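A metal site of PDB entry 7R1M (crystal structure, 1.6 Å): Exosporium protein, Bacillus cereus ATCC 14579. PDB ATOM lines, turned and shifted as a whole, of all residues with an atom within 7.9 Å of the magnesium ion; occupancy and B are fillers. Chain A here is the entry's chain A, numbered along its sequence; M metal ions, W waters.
The side-chain carboxylate (OE2) of Glu 96 is in hydrogen-bond range of the backbone NH (N) of Asn 90, at 3.1 Å.
The nearest printed residue that does not touch the magnesium ion is Asn 90 (4.2 Å).
OD1 of Asp 89 binds the magnesium ion (1.8 Å).
The magnesium ion is bound by water W3 (1.8 Å).
Water W2 is bound to the magnesium ion.
The backbone carbonyl oxygen (O) of Val 91 is bound to the magnesium ion (2.2 Å).
The magnesium ion is bound by water W1 (2.2 Å).
OE1 of Glu 96 is bound to the magnesium ion.
The magnesium ion has six donor atoms within binding distance.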
ATOM      1  N   PHE A  37      21.374  19.589  23.921  1.00  0.00           N
ATOM      2  CA  PHE A  37      20.861  20.539  24.925  1.00  0.00           C
ATOM      3  C   PHE A  37      21.935  21.594  25.176  1.00  0.00           C
ATOM      4  O   PHE A  37      23.088  21.238  25.327  1.00  0.00           O
ATOM      5  CB  PHE A  37      20.482  19.844  26.230  1.00  0.00           C
ATOM      6  CG  PHE A  37      19.295  18.926  26.100  1.00  0.00           C
ATOM      7  CD1 PHE A  37      18.039  19.444  25.790  1.00  0.00           C
ATOM      8  CD2 PHE A  37      19.432  17.563  26.312  1.00  0.00           C
ATOM      9  CE1 PHE A  37      16.947  18.609  25.671  1.00  0.00           C
ATOM     10  CE2 PHE A  37      18.332  16.730  26.167  1.00  0.00           C
ATOM     11  CZ  PHE A  37      17.089  17.246  25.860  1.00  0.00           C
ATOM     12  N   ILE A  86      15.848  26.263  17.599  1.00  0.00           N
ATOM     13  CA  ILE A  86      15.526  25.800  18.960  1.00  0.00           C
ATOM     14  C   ILE A  86      14.113  25.234  18.908  1.00  0.00           C
ATOM     15  O   ILE A  86      13.240  25.863  18.290  1.00  0.00           O
ATOM     16  CB  ILE A  86      15.672  26.946  19.974  1.00  0.00           C
ATOM     17  CG1 ILE A  86      17.124  27.415  20.089  1.00  0.00           C
ATOM     18  CG2 ILE A  86      15.135  26.514  21.331  1.00  0.00           C
ATOM     19  CD1 ILE A  86      17.496  28.448  19.090  1.00  0.00           C
ATOM     20  N   SER A  87      13.922  24.047  19.505  1.00  0.00           N
ATOM     21  CA  SER A  87      12.573  23.464  19.625  1.00  0.00           C
ATOM     22  C   SER A  87      11.972  23.950  20.942  1.00  0.00           C
ATOM     23  O   SER A  87      12.473  23.554  21.991  1.00  0.00           O
ATOM     24  CB  SER A  87      12.623  21.961  19.575  1.00  0.00           C
ATOM     25  OG  SER A  87      11.342  21.403  19.824  1.00  0.00           O
ATOM     26  N   LEU A  88      10.950  24.794  20.861  1.00  0.00           N
ATOM     27  CA  LEU A  88      10.315  25.367  22.082  1.00  0.00           C
ATOM     28  C   LEU A  88       9.038  24.598  22.398  1.00  0.00           C
ATOM     29  O   LEU A  88       8.184  24.472  21.496  1.00  0.00           O
ATOM     30  CB  LEU A  88      10.024  26.853  21.836  1.00  0.00           C
ATOM     31  CG  LEU A  88      11.252  27.762  21.775  1.00  0.00           C
ATOM     32  CD1 LEU A  88      10.856  29.191  21.471  1.00  0.00           C
ATOM     33  CD2 LEU A  88      12.041  27.685  23.072  1.00  0.00           C
ATOM     34  N   ASP A  89       8.902  24.111  23.631  1.00  0.00           N
ATOM     35  CA  ASP A  89       7.702  23.318  24.025  1.00  0.00           C
ATOM     36  C   ASP A  89       7.380  23.560  25.504  1.00  0.00           C
ATOM     37  O   ASP A  89       6.370  23.011  25.972  1.00  0.00           O
ATOM     38  CB  ASP A  89       7.904  21.833  23.741  1.00  0.00           C
ATOM     39  CG  ASP A  89       9.041  21.198  24.512  1.00  0.00           C
ATOM     40  OD1 ASP A  89       9.595  21.873  25.411  1.00  0.00           O
ATOM     41  OD2 ASP A  89       9.367  20.027  24.223  1.00  0.00           O
ATOM     42  N   ASN A  90       8.205  24.333  26.211  1.00  0.00           N
ATOM     43  CA  ASN A  90       7.960  24.644  27.647  1.00  0.00           C
ATOM     44  C   ASN A  90       7.939  23.348  28.473  1.00  0.00           C
ATOM     45  O   ASN A  90       7.246  23.325  29.505  1.00  0.00           O
ATOM     46  CB  ASN A  90       6.690  25.466  27.838  1.00  0.00           C
ATOM     47  CG  ASN A  90       6.817  26.873  27.283  1.00  0.00           C
ATOM     48  OD1 ASN A  90       7.922  27.410  27.208  1.00  0.00           O
ATOM     49  ND2 ASN A  90       5.706  27.464  26.887  1.00  0.00           N
ATOM     50  N   VAL A  91       8.663  22.321  28.021  1.00  0.00           N
ATOM     51  CA  VAL A  91       8.744  21.036  28.777  1.00  0.00           C
ATOM     52  C   VAL A  91      10.212  20.605  28.831  1.00  0.00           C
ATOM     53  O   VAL A  91      10.854  20.580  27.761  1.00  0.00           O
ATOM     54  CB  VAL A  91       7.865  19.950  28.121  1.00  0.00           C
ATOM     55  CG1 VAL A  91       8.125  18.568  28.702  1.00  0.00           C
ATOM     56  CG2 VAL A  91       6.383  20.305  28.186  1.00  0.00           C
ATOM     57  N   PRO A  92      10.782  20.288  30.012  1.00  0.00           N
ATOM     58  CA  PRO A  92       9.985  19.886  31.171  1.00  0.00           C
ATOM     59  C   PRO A  92       9.507  21.081  32.002  1.00  0.00           C
ATOM     60  O   PRO A  92       8.669  20.905  32.862  1.00  0.00           O
ATOM     61  CB  PRO A  92      11.009  19.096  31.999  1.00  0.00           C
ATOM     62  CG  PRO A  92      12.316  19.816  31.730  1.00  0.00           C
ATOM     63  CD  PRO A  92      12.214  20.281  30.289  1.00  0.00           C
ATOM     64  N   THR A  93      10.054  22.278  31.738  1.00  0.00           N
ATOM     65  CA  THR A  93       9.696  23.470  32.544  1.00  0.00           C
ATOM     66  C   THR A  93       9.493  24.676  31.629  1.00  0.00           C
ATOM     67  O   THR A  93       9.944  24.632  30.470  1.00  0.00           O
ATOM     68  CB  THR A  93      10.793  23.795  33.575  1.00  0.00           C
ATOM     69  OG1 THR A  93      12.001  24.055  32.862  1.00  0.00           O
ATOM     70  CG2 THR A  93      11.011  22.672  34.573  1.00  0.00           C
ATOM     71  N   GLU A  96      11.329  28.501  28.402  1.00  0.00           N
ATOM     72  CA  GLU A  96      12.619  28.040  27.826  1.00  0.00           C
ATOM     73  C   GLU A  96      13.234  29.235  27.108  1.00  0.00           C
ATOM     74  O   GLU A  96      12.598  29.756  26.177  1.00  0.00           O
ATOM     75  CB  GLU A  96      12.407  26.864  26.875  1.00  0.00           C
ATOM     76  CG  GLU A  96      11.891  25.609  27.557  1.00  0.00           C
ATOM     77  CD  GLU A  96      11.580  24.447  26.632  1.00  0.00           C
ATOM     78  OE1 GLU A  96      11.663  23.293  27.076  1.00  0.00           O
ATOM     79  OE2 GLU A  96      11.236  24.710  25.465  1.00  0.00           O
ATOM     80  N   GLY A 154      15.514  27.159  31.842  1.00  0.00           N
ATOM     81  CA  GLY A 154      14.849  25.921  31.405  1.00  0.00           C
ATOM     82  C   GLY A 154      15.772  25.046  30.564  1.00  0.00           C
ATOM     83  O   GLY A 154      16.992  25.291  30.597  1.00  0.00           O
ATOM     84  N   THR A 155      15.213  24.073  29.856  1.00  0.00           N
ATOM     85  CA  THR A 155      16.036  23.149  29.029  1.00  0.00           C
ATOM     86  C   THR A 155      15.976  23.614  27.560  1.00  0.00           C
ATOM     87  O   THR A 155      14.891  23.538  26.965  1.00  0.00           O
ATOM     88  CB  THR A 155      15.569  21.704  29.207  1.00  0.00           C
ATOM     89  OG1 THR A 155      15.711  21.368  30.591  1.00  0.00           O
ATOM     90  CG2 THR A 155      16.352  20.725  28.352  1.00  0.00           C
ATOM     91  N   VAL A 156      17.112  24.070  27.024  1.00  0.00           N
ATOM     92  CA  VAL A 156      17.148  24.591  25.624  1.00  0.00           C
ATOM     93  C   VAL A 156      17.526  23.447  24.666  1.00  0.00           C
ATOM     94  O   VAL A 156      18.668  22.981  24.739  1.00  0.00           O
ATOM     95  CB  VAL A 156      18.041  25.823  25.475  1.00  0.00           C
ATOM     96  CG1 VAL A 156      18.128  26.282  24.025  1.00  0.00           C
ATOM     97  CG2 VAL A 156      17.554  26.963  26.364  1.00  0.00           C
ATOM     98  N   ASP A 157      16.595  23.043  23.823  1.00  0.00           N
ATOM     99  CA  ASP A 157      16.738  21.925  22.852  1.00  0.00           C
ATOM    100  C   ASP A 157      17.131  22.530  21.491  1.00  0.00           C
ATOM    101  O   ASP A 157      16.301  23.190  20.817  1.00  0.00           O
ATOM    102  CB  ASP A 157      15.472  21.090  22.870  1.00  0.00           C
ATOM    103  CG  ASP A 157      15.530  19.822  22.058  1.00  0.00           C
ATOM    104  OD1 ASP A 157      16.460  19.675  21.238  1.00  0.00           O
ATOM    105  OD2 ASP A 157      14.633  18.946  22.268  1.00  0.00           O
ATOM    106  N   ARG A 159      18.010  22.118  17.763  1.00  0.00           N
ATOM    107  CA  ARG A 159      17.802  21.152  16.668  1.00  0.00           C
ATOM    108  C   ARG A 159      18.663  21.455  15.459  1.00  0.00           C
ATOM    109  O   ARG A 159      18.685  20.645  14.546  1.00  0.00           O
ATOM    110  CB  ARG A 159      16.320  21.142  16.287  1.00  0.00           C
ATOM    111  CG  ARG A 159      15.450  20.623  17.426  1.00  0.00           C
ATOM    112  CD  ARG A 159      15.721  19.149  17.663  1.00  0.00           C
ATOM    113  NE  ARG A 159      15.220  18.679  18.947  1.00  0.00           N
ATOM    114  CZ  ARG A 159      14.930  17.418  19.251  1.00  0.00           C
ATOM    115  NH1 ARG A 159      15.042  16.448  18.351  1.00  0.00           N
ATOM    116  NH2 ARG A 159      14.516  17.110  20.465  1.00  0.00           N
HETATM  117 MG    MG M   1      11.288  21.456  25.832  1.00  0.00          MG
HETATM  118  O   HOH W   1      13.335  21.056  26.460  1.00  0.00           O
HETATM  119  O   HOH W   2      11.458  19.603  25.520  1.00  0.00           O
HETATM  120  O   HOH W   3      12.003  21.897  24.188  1.00  0.00           O
